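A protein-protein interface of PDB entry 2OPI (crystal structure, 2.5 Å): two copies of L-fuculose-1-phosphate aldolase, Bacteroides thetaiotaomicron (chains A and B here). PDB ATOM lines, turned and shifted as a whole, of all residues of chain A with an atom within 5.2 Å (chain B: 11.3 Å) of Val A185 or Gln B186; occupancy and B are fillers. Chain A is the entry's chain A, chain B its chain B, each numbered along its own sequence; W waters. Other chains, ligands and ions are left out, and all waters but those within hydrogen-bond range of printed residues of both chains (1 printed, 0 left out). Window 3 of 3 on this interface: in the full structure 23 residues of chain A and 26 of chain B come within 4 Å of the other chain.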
ATOM      1  N   GLU A  97     -24.167  11.528 -26.446  1.00  0.00           N
ATOM      2  CA  GLU A  97     -24.066  10.101 -26.806  1.00  0.00           C
ATOM      3  C   GLU A  97     -22.865   9.325 -26.212  1.00  0.00           C
ATOM      4  O   GLU A  97     -23.002   8.656 -25.185  1.00  0.00           O
ATOM      5  CB  GLU A  97     -24.059   9.991 -28.331  1.00  0.00           C
ATOM      6  CG  GLU A  97     -24.379   8.616 -28.913  1.00  0.00           C
ATOM      7  CD  GLU A  97     -24.740   8.700 -30.396  1.00  0.00           C
ATOM      8  OE1 GLU A  97     -25.131   7.678 -30.999  1.00  0.00           O
ATOM      9  OE2 GLU A  97     -24.647   9.803 -30.962  1.00  0.00           O
ATOM     10  N   TYR A  98     -21.701   9.415 -26.854  1.00  0.00           N
ATOM     11  CA  TYR A  98     -20.583   8.534 -26.526  1.00  0.00           C
ATOM     12  C   TYR A  98     -19.899   8.901 -25.211  1.00  0.00           C
ATOM     13  O   TYR A  98     -19.328   8.040 -24.536  1.00  0.00           O
ATOM     14  CB  TYR A  98     -19.571   8.468 -27.678  1.00  0.00           C
ATOM     15  CG  TYR A  98     -20.066   7.701 -28.891  1.00  0.00           C
ATOM     16  CD1 TYR A  98     -20.806   8.329 -29.900  1.00  0.00           C
ATOM     17  CD2 TYR A  98     -19.799   6.348 -29.024  1.00  0.00           C
ATOM     18  CE1 TYR A  98     -21.279   7.614 -31.001  1.00  0.00           C
ATOM     19  CE2 TYR A  98     -20.254   5.628 -30.110  1.00  0.00           C
ATOM     20  CZ  TYR A  98     -20.989   6.254 -31.095  1.00  0.00           C
ATOM     21  OH  TYR A  98     -21.406   5.503 -32.178  1.00  0.00           O
ATOM     22  N   ALA A 101     -21.931   7.254 -22.387  1.00  0.00           N
ATOM     23  CA  ALA A 101     -21.537   5.848 -22.367  1.00  0.00           C
ATOM     24  C   ALA A 101     -20.258   5.666 -21.542  1.00  0.00           C
ATOM     25  O   ALA A 101     -20.176   4.766 -20.698  1.00  0.00           O
ATOM     26  CB  ALA A 101     -21.328   5.337 -23.778  1.00  0.00           C
ATOM     27  N   ILE A 102     -19.271   6.528 -21.796  1.00  0.00           N
ATOM     28  CA  ILE A 102     -18.043   6.583 -21.011  1.00  0.00           C
ATOM     29  C   ILE A 102     -18.332   6.948 -19.547  1.00  0.00           C
ATOM     30  O   ILE A 102     -17.704   6.394 -18.654  1.00  0.00           O
ATOM     31  CB  ILE A 102     -16.998   7.559 -21.629  1.00  0.00           C
ATOM     32  CG1 ILE A 102     -16.605   7.127 -23.043  1.00  0.00           C
ATOM     33  CG2 ILE A 102     -15.755   7.719 -20.733  1.00  0.00           C
ATOM     34  CD1 ILE A 102     -15.498   6.154 -23.127  1.00  0.00           C
ATOM     35  N   MET A 105     -19.380   3.749 -17.738  1.00  0.00           N
ATOM     36  CA  MET A 105     -18.427   2.631 -17.821  1.00  0.00           C
ATOM     37  C   MET A 105     -17.777   2.329 -16.491  1.00  0.00           C
ATOM     38  O   MET A 105     -17.367   3.236 -15.779  1.00  0.00           O
ATOM     39  CB  MET A 105     -17.317   2.920 -18.825  1.00  0.00           C
ATOM     40  CG  MET A 105     -17.687   2.656 -20.253  1.00  0.00           C
ATOM     41  SD  MET A 105     -16.105   2.666 -21.409  1.00  0.00           S
ATOM     42  CE  MET A 105     -17.041   2.512 -23.122  1.00  0.00           C
ATOM     43  N   CYS A 181     -14.542  10.835 -26.969  1.00  0.00           N
ATOM     44  CA  CYS A 181     -15.275   9.662 -26.527  1.00  0.00           C
ATOM     45  C   CYS A 181     -15.779   8.796 -27.673  1.00  0.00           C
ATOM     46  O   CYS A 181     -15.719   7.570 -27.582  1.00  0.00           O
ATOM     47  CB  CYS A 181     -16.429  10.083 -25.639  1.00  0.00           C
ATOM     48  SG  CYS A 181     -15.829  10.851 -24.137  1.00  0.00           S
ATOM     49  N   ARG A 182     -16.256   9.427 -28.744  1.00  0.00           N
ATOM     50  CA  ARG A 182     -16.732   8.687 -29.914  1.00  0.00           C
ATOM     51  C   ARG A 182     -15.611   7.882 -30.549  1.00  0.00           C
ATOM     52  O   ARG A 182     -15.815   6.731 -30.937  1.00  0.00           O
ATOM     53  CB  ARG A 182     -17.390   9.625 -30.932  1.00  0.00           C
ATOM     54  CG  ARG A 182     -17.887   8.948 -32.210  1.00  0.00           C
ATOM     55  CD  ARG A 182     -18.827   9.835 -33.033  1.00  0.00           C
ATOM     56  NE  ARG A 182     -18.461  11.263 -33.045  1.00  0.00           N
ATOM     57  CZ  ARG A 182     -17.489  11.800 -33.792  1.00  0.00           C
ATOM     58  NH1 ARG A 182     -16.739  11.042 -34.594  1.00  0.00           N
ATOM     59  NH2 ARG A 182     -17.258  13.108 -33.730  1.00  0.00           N
ATOM     60  N   ILE A 183     -14.424   8.481 -30.624  1.00  0.00           N
ATOM     61  CA  ILE A 183     -13.237   7.780 -31.121  1.00  0.00           C
ATOM     62  C   ILE A 183     -12.935   6.557 -30.255  1.00  0.00           C
ATOM     63  O   ILE A 183     -12.776   5.460 -30.776  1.00  0.00           O
ATOM     64  CB  ILE A 183     -11.976   8.692 -31.170  1.00  0.00           C
ATOM     65  CG1 ILE A 183     -12.129   9.853 -32.174  1.00  0.00           C
ATOM     66  CG2 ILE A 183     -10.740   7.884 -31.476  1.00  0.00           C
ATOM     67  CD1 ILE A 183     -12.874   9.503 -33.445  1.00  0.00           C
ATOM     68  N   ILE A 184     -12.867   6.748 -28.938  1.00  0.00           N
ATOM     69  CA  ILE A 184     -12.519   5.660 -28.037  1.00  0.00           C
ATOM     70  C   ILE A 184     -13.461   4.463 -28.236  1.00  0.00           C
ATOM     71  O   ILE A 184     -13.005   3.320 -28.363  1.00  0.00           O
ATOM     72  CB  ILE A 184     -12.573   6.075 -26.544  1.00  0.00           C
ATOM     73  CG1 ILE A 184     -11.754   7.347 -26.244  1.00  0.00           C
ATOM     74  CG2 ILE A 184     -12.186   4.904 -25.634  1.00  0.00           C
ATOM     75  CD1 ILE A 184     -10.331   7.338 -26.675  1.00  0.00           C
ATOM     76  N   VAL A 185     -14.765   4.729 -28.272  1.00  0.00           N
ATOM     77  CA  VAL A 185     -15.747   3.654 -28.337  1.00  0.00           C
ATOM     78  C   VAL A 185     -15.730   2.976 -29.706  1.00  0.00           C
ATOM     79  O   VAL A 185     -15.699   1.747 -29.803  1.00  0.00           O
ATOM     80  CB  VAL A 185     -17.166   4.146 -28.011  1.00  0.00           C
ATOM     81  CG1 VAL A 185     -18.166   3.009 -28.155  1.00  0.00           C
ATOM     82  CG2 VAL A 185     -17.230   4.756 -26.607  1.00  0.00           C
ATOM     83  N   GLN A 186     -15.725   3.774 -30.766  1.00  0.00           N
ATOM     84  CA  GLN A 186     -15.798   3.202 -32.107  1.00  0.00           C
ATOM     85  C   GLN A 186     -14.539   2.419 -32.463  1.00  0.00           C
ATOM     86  O   GLN A 186     -14.615   1.455 -33.205  1.00  0.00           O
ATOM     87  CB  GLN A 186     -16.145   4.271 -33.152  1.00  0.00           C
ATOM     88  CG  GLN A 186     -17.607   4.762 -33.044  1.00  0.00           C
ATOM     89  CD  GLN A 186     -17.947   5.862 -34.034  1.00  0.00           C
ATOM     90  OE1 GLN A 186     -17.061   6.484 -34.622  1.00  0.00           O
ATOM     91  NE2 GLN A 186     -19.236   6.114 -34.217  1.00  0.00           N
ATOM     92  N   SER A 187     -13.395   2.806 -31.909  1.00  0.00           N
ATOM     93  CA  SER A 187     -12.144   2.091 -32.125  1.00  0.00           C
ATOM     94  C   SER A 187     -12.140   0.719 -31.471  1.00  0.00           C
ATOM     95  O   SER A 187     -11.303  -0.122 -31.780  1.00  0.00           O
ATOM     96  CB  SER A 187     -10.956   2.916 -31.612  1.00  0.00           C
ATOM     97  OG  SER A 187     -10.950   2.996 -30.194  1.00  0.00           O
ATOM     98  N   GLY A 188     -13.070   0.509 -30.548  1.00  0.00           N
ATOM     99  CA  GLY A 188     -13.205  -0.767 -29.856  1.00  0.00           C
ATOM    100  C   GLY A 188     -12.222  -0.929 -28.716  1.00  0.00           C
ATOM    101  O   GLY A 188     -11.899  -2.052 -28.324  1.00  0.00           O
ATOM    102  N   GLY A 189     -11.734   0.192 -28.197  1.00  0.00           N
ATOM    103  CA  GLY A 189     -10.795   0.175 -27.082  1.00  0.00           C
ATOM    104  C   GLY A 189      -9.322   0.058 -27.449  1.00  0.00           C
ATOM    105  O   GLY A 189      -8.450   0.281 -26.604  1.00  0.00           O
ATOM    106  N   GLU B  97     -34.086   2.707 -31.922  1.00  0.00           N
ATOM    107  CA  GLU B  97     -32.876   2.083 -32.441  1.00  0.00           C
ATOM    108  C   GLU B  97     -32.248   1.084 -31.454  1.00  0.00           C
ATOM    109  O   GLU B  97     -32.316  -0.121 -31.661  1.00  0.00           O
ATOM    110  CB  GLU B  97     -31.873   3.167 -32.844  1.00  0.00           C
ATOM    111  CG  GLU B  97     -30.558   2.636 -33.382  1.00  0.00           C
ATOM    112  CD  GLU B  97     -29.665   3.734 -33.908  1.00  0.00           C
ATOM    113  OE1 GLU B  97     -28.575   3.424 -34.425  1.00  0.00           O
ATOM    114  OE2 GLU B  97     -30.046   4.912 -33.807  1.00  0.00           O
ATOM    115  N   TYR B  98     -31.650   1.588 -30.381  1.00  0.00           N
ATOM    116  CA  TYR B  98     -30.870   0.747 -29.487  1.00  0.00           C
ATOM    117  C   TYR B  98     -31.750  -0.087 -28.581  1.00  0.00           C
ATOM    118  O   TYR B  98     -31.353  -1.172 -28.156  1.00  0.00           O
ATOM    119  CB  TYR B  98     -29.867   1.582 -28.672  1.00  0.00           C
ATOM    120  CG  TYR B  98     -28.659   2.016 -29.482  1.00  0.00           C
ATOM    121  CD1 TYR B  98     -28.654   3.232 -30.165  1.00  0.00           C
ATOM    122  CD2 TYR B  98     -27.535   1.205 -29.585  1.00  0.00           C
ATOM    123  CE1 TYR B  98     -27.559   3.634 -30.924  1.00  0.00           C
ATOM    124  CE2 TYR B  98     -26.427   1.600 -30.346  1.00  0.00           C
ATOM    125  CZ  TYR B  98     -26.452   2.817 -31.010  1.00  0.00           C
ATOM    126  OH  TYR B  98     -25.375   3.224 -31.766  1.00  0.00           O
ATOM    127  N   ALA B  99     -32.944   0.424 -28.303  1.00  0.00           N
ATOM    128  CA  ALA B  99     -33.894  -0.263 -27.453  1.00  0.00           C
ATOM    129  C   ALA B  99     -34.463  -1.476 -28.164  1.00  0.00           C
ATOM    130  O   ALA B  99     -34.751  -2.467 -27.525  1.00  0.00           O
ATOM    131  CB  ALA B  99     -34.980   0.669 -26.999  1.00  0.00           C
ATOM    132  N   ALA B 101     -32.662  -3.132 -30.543  1.00  0.00           N
ATOM    133  CA  ALA B 101     -31.506  -4.021 -30.519  1.00  0.00           C
ATOM    134  C   ALA B 101     -31.528  -4.851 -29.224  1.00  0.00           C
ATOM    135  O   ALA B 101     -31.410  -6.085 -29.246  1.00  0.00           O
ATOM    136  CB  ALA B 101     -30.208  -3.238 -30.638  1.00  0.00           C
ATOM    137  N   ILE B 102     -31.689  -4.163 -28.106  1.00  0.00           N
ATOM    138  CA  ILE B 102     -31.704  -4.797 -26.811  1.00  0.00           C
ATOM    139  C   ILE B 102     -32.885  -5.761 -26.672  1.00  0.00           C
ATOM    140  O   ILE B 102     -32.746  -6.824 -26.055  1.00  0.00           O
ATOM    141  CB  ILE B 102     -31.702  -3.741 -25.690  1.00  0.00           C
ATOM    142  CG1 ILE B 102     -30.291  -3.185 -25.523  1.00  0.00           C
ATOM    143  CG2 ILE B 102     -32.223  -4.325 -24.384  1.00  0.00           C
ATOM    144  CD1 ILE B 102     -30.117  -2.356 -24.274  1.00  0.00           C
ATOM    145  N   MET B 105     -31.786  -8.983 -28.057  1.00  0.00           N
ATOM    146  CA  MET B 105     -30.611  -9.597 -27.461  1.00  0.00           C
ATOM    147  C   MET B 105     -30.965 -10.786 -26.591  1.00  0.00           C
ATOM    148  O   MET B 105     -31.983 -10.787 -25.910  1.00  0.00           O
ATOM    149  CB  MET B 105     -29.846  -8.573 -26.642  1.00  0.00           C
ATOM    150  CG  MET B 105     -28.585  -8.101 -27.302  1.00  0.00           C
ATOM    151  SD  MET B 105     -27.972  -6.390 -26.533  1.00  0.00           S
ATOM    152  CE  MET B 105     -28.372  -5.260 -28.074  1.00  0.00           C
ATOM    153  N   PRO B 109     -30.298  -6.687 -20.191  1.00  0.00           N
ATOM    154  CA  PRO B 109     -29.991  -6.048 -18.916  1.00  0.00           C
ATOM    155  C   PRO B 109     -30.931  -6.473 -17.802  1.00  0.00           C
ATOM    156  O   PRO B 109     -32.125  -6.661 -18.019  1.00  0.00           O
ATOM    157  CB  PRO B 109     -30.221  -4.567 -19.205  1.00  0.00           C
ATOM    158  CG  PRO B 109     -29.983  -4.428 -20.644  1.00  0.00           C
ATOM    159  CD  PRO B 109     -30.464  -5.693 -21.272  1.00  0.00           C
ATOM    160  N   VAL B 114     -28.853   3.659 -15.332  1.00  0.00           N
ATOM    161  CA  VAL B 114     -27.488   4.102 -15.604  1.00  0.00           C
ATOM    162  C   VAL B 114     -27.250   5.595 -15.361  1.00  0.00           C
ATOM    163  O   VAL B 114     -26.114   6.001 -15.118  1.00  0.00           O
ATOM    164  CB  VAL B 114     -27.019   3.669 -16.999  1.00  0.00           C
ATOM    165  CG1 VAL B 114     -26.913   2.149 -17.048  1.00  0.00           C
ATOM    166  CG2 VAL B 114     -27.968   4.194 -18.089  1.00  0.00           C
ATOM    167  N   THR B 115     -28.303   6.407 -15.426  1.00  0.00           N
ATOM    168  CA  THR B 115     -28.220   7.813 -15.035  1.00  0.00           C
ATOM    169  C   THR B 115     -29.446   8.134 -14.193  1.00  0.00           C
ATOM    170  O   THR B 115     -30.358   7.315 -14.098  1.00  0.00           O
ATOM    171  CB  THR B 115     -28.175   8.793 -16.243  1.00  0.00           C
ATOM    172  OG1 THR B 115     -29.474   8.890 -16.833  1.00  0.00           O
ATOM    173  CG2 THR B 115     -27.180   8.360 -17.297  1.00  0.00           C
ATOM    174  N   THR B 175     -37.519   8.910 -25.165  1.00  0.00           N
ATOM    175  CA  THR B 175     -36.143   9.293 -25.471  1.00  0.00           C
ATOM    176  C   THR B 175     -35.154   8.744 -24.459  1.00  0.00           C
ATOM    177  O   THR B 175     -34.045   8.362 -24.826  1.00  0.00           O
ATOM    178  CB  THR B 175     -35.963  10.820 -25.465  1.00  0.00           C
ATOM    179  OG1 THR B 175     -37.065  11.447 -26.118  1.00  0.00           O
ATOM    180  CG2 THR B 175     -34.688  11.217 -26.183  1.00  0.00           C
ATOM    181  N   PHE B 177     -35.700   6.113 -22.463  1.00  0.00           N
ATOM    182  CA  PHE B 177     -35.746   4.674 -22.600  1.00  0.00           C
ATOM    183  C   PHE B 177     -34.704   4.329 -23.671  1.00  0.00           C
ATOM    184  O   PHE B 177     -33.840   3.468 -23.464  1.00  0.00           O
ATOM    185  CB  PHE B 177     -37.157   4.269 -23.039  1.00  0.00           C
ATOM    186  CG  PHE B 177     -37.500   2.816 -22.830  1.00  0.00           C
ATOM    187  CD1 PHE B 177     -36.522   1.827 -22.825  1.00  0.00           C
ATOM    188  CD2 PHE B 177     -38.834   2.440 -22.686  1.00  0.00           C
ATOM    189  CE1 PHE B 177     -36.865   0.482 -22.638  1.00  0.00           C
ATOM    190  CE2 PHE B 177     -39.198   1.113 -22.510  1.00  0.00           C
ATOM    191  CZ  PHE B 177     -38.211   0.119 -22.490  1.00  0.00           C
ATOM    192  N   GLU B 178     -34.771   5.037 -24.796  1.00  0.00           N
ATOM    193  CA  GLU B 178     -33.806   4.879 -25.876  1.00  0.00           C
ATOM    194  C   GLU B 178     -32.382   5.198 -25.433  1.00  0.00           C
ATOM    195  O   GLU B 178     -31.441   4.482 -25.786  1.00  0.00           O
ATOM    196  CB  GLU B 178     -34.197   5.734 -27.084  1.00  0.00           C
ATOM    197  CG  GLU B 178     -33.214   5.679 -28.262  1.00  0.00           C
ATOM    198  CD  GLU B 178     -32.867   4.250 -28.730  1.00  0.00           C
ATOM    199  OE1 GLU B 178     -33.615   3.285 -28.413  1.00  0.00           O
ATOM    200  OE2 GLU B 178     -31.840   4.089 -29.435  1.00  0.00           O
ATOM    201  N   MET B 179     -32.213   6.259 -24.656  1.00  0.00           N
ATOM    202  CA  MET B 179     -30.876   6.627 -24.214  1.00  0.00           C
ATOM    203  C   MET B 179     -30.217   5.581 -23.295  1.00  0.00           C
ATOM    204  O   MET B 179     -29.048   5.252 -23.477  1.00  0.00           O
ATOM    205  CB  MET B 179     -30.880   8.002 -23.576  1.00  0.00           C
ATOM    206  CG  MET B 179     -29.536   8.394 -23.038  1.00  0.00           C
ATOM    207  SD  MET B 179     -29.616  10.000 -21.944  1.00  0.00           S
ATOM    208  CE  MET B 179     -28.511  11.167 -23.068  1.00  0.00           C
ATOM    209  N   ALA B 180     -30.964   5.072 -22.312  1.00  0.00           N
ATOM    210  CA  ALA B 180     -30.490   3.976 -21.456  1.00  0.00           C
ATOM    211  C   ALA B 180     -29.983   2.817 -22.303  1.00  0.00           C
ATOM    212  O   ALA B 180     -28.860   2.351 -22.126  1.00  0.00           O
ATOM    213  CB  ALA B 180     -31.565   3.510 -20.528  1.00  0.00           C
ATOM    214  N   CYS B 181     -30.787   2.391 -23.266  1.00  0.00           N
ATOM    215  CA  CYS B 181     -30.367   1.322 -24.151  1.00  0.00           C
ATOM    216  C   CYS B 181     -29.127   1.662 -24.954  1.00  0.00           C
ATOM    217  O   CYS B 181     -28.260   0.799 -25.142  1.00  0.00           O
ATOM    218  CB  CYS B 181     -31.500   0.928 -25.080  1.00  0.00           C
ATOM    219  SG  CYS B 181     -32.850   0.322 -24.163  1.00  0.00           S
ATOM    220  N   ARG B 182     -29.049   2.902 -25.433  1.00  0.00           N
ATOM    221  CA  ARG B 182     -27.867   3.374 -26.156  1.00  0.00           C
ATOM    222  C   ARG B 182     -26.591   3.289 -25.313  1.00  0.00           C
ATOM    223  O   ARG B 182     -25.557   2.831 -25.809  1.00  0.00           O
ATOM    224  CB  ARG B 182     -28.092   4.791 -26.668  1.00  0.00           C
ATOM    225  CG  ARG B 182     -27.072   5.292 -27.662  1.00  0.00           C
ATOM    226  CD  ARG B 182     -27.231   6.788 -27.909  1.00  0.00           C
ATOM    227  NE  ARG B 182     -28.577   7.089 -28.378  1.00  0.00           N
ATOM    228  CZ  ARG B 182     -29.388   8.012 -27.864  1.00  0.00           C
ATOM    229  NH1 ARG B 182     -28.994   8.794 -26.862  1.00  0.00           N
ATOM    230  NH2 ARG B 182     -30.598   8.169 -28.383  1.00  0.00           N
ATOM    231  N   ILE B 183     -26.671   3.709 -24.047  1.00  0.00           N
ATOM    232  CA  ILE B 183     -25.553   3.631 -23.095  1.00  0.00           C
ATOM    233  C   ILE B 183     -25.101   2.184 -22.926  1.00  0.00           C
ATOM    234  O   ILE B 183     -23.911   1.891 -22.933  1.00  0.00           O
ATOM    235  CB  ILE B 183     -25.952   4.169 -21.660  1.00  0.00           C
ATOM    236  CG1 ILE B 183     -26.589   5.577 -21.685  1.00  0.00           C
ATOM    237  CG2 ILE B 183     -24.797   4.098 -20.680  1.00  0.00           C
ATOM    238  CD1 ILE B 183     -25.684   6.672 -22.041  1.00  0.00           C
ATOM    239  N   ILE B 184     -26.059   1.283 -22.769  1.00  0.00           N
ATOM    240  CA  ILE B 184     -25.770  -0.111 -22.505  1.00  0.00           C
ATOM    241  C   ILE B 184     -25.074  -0.799 -23.686  1.00  0.00           C
ATOM    242  O   ILE B 184     -24.043  -1.466 -23.509  1.00  0.00           O
ATOM    243  CB  ILE B 184     -27.062  -0.852 -22.064  1.00  0.00           C
ATOM    244  CG1 ILE B 184     -27.537  -0.279 -20.712  1.00  0.00           C
ATOM    245  CG2 ILE B 184     -26.862  -2.383 -22.023  1.00  0.00           C
ATOM    246  CD1 ILE B 184     -29.011  -0.505 -20.438  1.00  0.00           C
ATOM    247  N   VAL B 185     -25.616  -0.628 -24.882  1.00  0.00           N
ATOM    248  CA  VAL B 185     -24.993  -1.201 -26.058  1.00  0.00           C
ATOM    249  C   VAL B 185     -23.603  -0.579 -26.258  1.00  0.00           C
ATOM    250  O   VAL B 185     -22.617  -1.303 -26.407  1.00  0.00           O
ATOM    251  CB  VAL B 185     -25.872  -1.004 -27.312  1.00  0.00           C
ATOM    252  CG1 VAL B 185     -25.130  -1.393 -28.585  1.00  0.00           C
ATOM    253  CG2 VAL B 185     -27.178  -1.766 -27.174  1.00  0.00           C
ATOM    254  N   GLN B 186     -23.523   0.750 -26.214  1.00  0.00           N
ATOM    255  CA  GLN B 186     -22.291   1.463 -26.585  1.00  0.00           C
ATOM    256  C   GLN B 186     -21.163   1.334 -25.569  1.00  0.00           C
ATOM    257  O   GLN B 186     -19.985   1.455 -25.928  1.00  0.00           O
ATOM    258  CB  GLN B 186     -22.563   2.940 -26.884  1.00  0.00           C
ATOM    259  CG  GLN B 186     -23.335   3.203 -28.196  1.00  0.00           C
ATOM    260  CD  GLN B 186     -23.610   4.688 -28.418  1.00  0.00           C
ATOM    261  OE1 GLN B 186     -23.502   5.496 -27.485  1.00  0.00           O
ATOM    262  NE2 GLN B 186     -23.970   5.055 -29.649  1.00  0.00           N
ATOM    263  N   SER B 187     -21.509   1.101 -24.304  1.00  0.00           N
ATOM    264  CA  SER B 187     -20.496   0.891 -23.278  1.00  0.00           C
ATOM    265  C   SER B 187     -19.901  -0.492 -23.455  1.00  0.00           C
ATOM    266  O   SER B 187     -18.820  -0.781 -22.943  1.00  0.00           O
ATOM    267  CB  SER B 187     -21.105   0.990 -21.896  1.00  0.00           C
ATOM    268  OG  SER B 187     -22.082  -0.015 -21.714  1.00  0.00           O
ATOM    269  N   GLY B 188     -20.620  -1.342 -24.185  1.00  0.00           N
ATOM    270  CA  GLY B 188     -20.221  -2.724 -24.377  1.00  0.00           C
ATOM    271  C   GLY B 188     -20.668  -3.587 -23.219  1.00  0.00           C
ATOM    272  O   GLY B 188     -20.092  -4.632 -22.983  1.00  0.00           O
ATOM    273  N   GLY B 189     -21.694  -3.146 -22.494  1.00  0.00           N
ATOM    274  CA  GLY B 189     -22.263  -3.917 -21.387  1.00  0.00           C
ATOM    275  C   GLY B 189     -21.502  -3.834 -20.071  1.00  0.00           C
ATOM    276  O   GLY B 189     -21.981  -4.314 -19.031  1.00  0.00           O
ATOM    277  N   ASP B 190     -20.317  -3.233 -20.091  1.00  0.00           N
ATOM    278  CA  ASP B 190     -19.549  -3.106 -18.856  1.00  0.00           C
ATOM    279  C   ASP B 190     -19.742  -1.744 -18.189  1.00  0.00           C
ATOM    280  O   ASP B 190     -18.832  -0.912 -18.139  1.00  0.00           O
ATOM    281  CB  ASP B 190     -18.070  -3.461 -19.056  1.00  0.00           C
ATOM    282  CG  ASP B 190     -17.525  -4.353 -17.924  1.00  0.00           C
ATOM    283  OD1 ASP B 190     -17.810  -4.051 -16.728  1.00  0.00           O
ATOM    284  OD2 ASP B 190     -16.820  -5.357 -18.228  1.00  0.00           O
ATOM    285  N   TYR B 191     -20.947  -1.548 -17.659  1.00  0.00           N
ATOM    286  CA  TYR B 191     -21.326  -0.312 -16.998  1.00  0.00           C
ATOM    287  C   TYR B 191     -21.690  -0.523 -15.537  1.00  0.00           C
ATOM    288  O   TYR B 191     -21.941  -1.647 -15.106  1.00  0.00           O
ATOM    289  CB  TYR B 191     -22.513   0.307 -17.720  1.00  0.00           C
ATOM    290  CG  TYR B 191     -23.745  -0.553 -17.728  1.00  0.00           C
ATOM    291  CD1 TYR B 191     -24.019  -1.397 -18.799  1.00  0.00           C
ATOM    292  CD2 TYR B 191     -24.649  -0.523 -16.658  1.00  0.00           C
ATOM    293  CE1 TYR B 191     -25.150  -2.190 -18.806  1.00  0.00           C
ATOM    294  CE2 TYR B 191     -25.787  -1.315 -16.655  1.00  0.00           C
ATOM    295  CZ  TYR B 191     -26.031  -2.144 -17.731  1.00  0.00           C
ATOM    296  OH  TYR B 191     -27.173  -2.911 -17.745  1.00  0.00           O
ATOM    297  N   SER B 192     -21.734   0.567 -14.779  1.00  0.00           N
ATOM    298  CA  SER B 192     -22.269   0.523 -13.436  1.00  0.00           C
ATOM    299  C   SER B 192     -23.641   1.229 -13.361  1.00  0.00           C
ATOM    300  O   SER B 192     -24.011   1.983 -14.265  1.00  0.00           O
ATOM    301  CB  SER B 192     -21.272   1.116 -12.449  1.00  0.00           C
ATOM    302  OG  SER B 192     -21.102   2.481 -12.716  1.00  0.00           O
HETATM  303  O   HOH W   1     -27.577   6.912 -32.967  1.00  0.00           O
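The side-chain carboxylate (OE1) of Glu A97 is in hydrogen-bond range of the side-chain amide nitrogen (NE2) of Gln B186.
Water W1 lies within hydrogen-bond range of OE1 of Glu A97 (3.2 Å) and OE2 of Glu B97 (3.3 Å).
Glu A97 touches just these residues of chain B: Arg B182 (3.5 Å) and Gln B186 (3.2 Å).
Of the printed residues of chain B, Met A105 touches Ser B187 (3.7 Å) and Asp B190 (3.6 Å).
No residue of chain B comes within 4 Å of Ile A184.
No residue of chain B comes within 4 Å of Ser A187.
Gly A188 touches none of the printed residues of chain B.
Ala B180 touches none of the printed residues of chain A.
Of the printed residues of chain A, Arg B182 touches Glu A97 (3.5 Å).
Printed residues of chain A within 4 Å of Ile B183: Ala A101 (3.8 Å).
Gln B186 touches just these residues of chain A: Glu A97, Tyr A98 and Val A185.
The nearest residue of chain A that does not touch Gln B186 is Ala A101 (4.1 Å).
Hydrophobic or aromatic side chains of chain A that line the printed part of chain B: Tyr A98, Met A105 and Val A185.
Of the 26 printed residues of chain B, 5 touch a printed residue of chain A.
Hydrophobic or aromatic side chains of chain B that line the printed part of chain A: Ile B183.
Among the printed residues, 7 pairs touch across the chains.
Among the printed residues, no Asp or Glu carboxylate lies within 4 Å of a Lys or Arg side-chain nitrogen of the other chain.
Glu A97 touches Gln B186, but with the chains exchanged Gln A186 does not touch Glu B97 (9.7 Å).
Tyr A98 touches Gln B186, but with the chains exchanged Gln A186 does not touch Tyr B98 (7.2 Å).
Ala A101 touches Ile B183, but with the chains exchanged Ile A183 does not touch Ala B101 (19.5 Å).
Met A105 touches Ser B187, but with the chains exchanged Ser A187 does not touch Met B105 (17.4 Å).
Positions printed for both chains: 97, 98, 101, 102, 105, 181, 182, 183, 184, 185, 186, 187, 188 and 189.
Of the 7 pairs that touch across the chains among the printed residues, none has its exchanged pair printed and touching as well.
CG of Glu A97 touches CD of Arg B182 (3.5 Å).
CZ of Tyr A98 touches NE2 of Gln B186, 3.5 Å away.
Ala A101 touches Ile B183.
Ser B187 touches Met A105.
CA of Met A105 touches O of Asp B190 (3.6 Å).
O of Gln B186 touches CG1 of Val A185, at 3.3 Å.
The side-chain hydroxyl (OG) of Ser B187 sits at hydrogen-bond distance from the backbone carbonyl oxygen (O) of Ile B183.
N of Gly B189 lies within hydrogen-bond range of OG of Ser B187, at 3.2 Å.
NE2 of Gln B186 sits at hydrogen-bond distance from OH of Tyr B98 (3.1 Å).
O of Ile B184 is in hydrogen-bond range of OG of Ser B187, 3.0 Å away.
The side-chain amide nitrogen (NE2) of Gln A186 sits at hydrogen-bond distance from the side-chain hydroxyl (OH) of Tyr A98.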
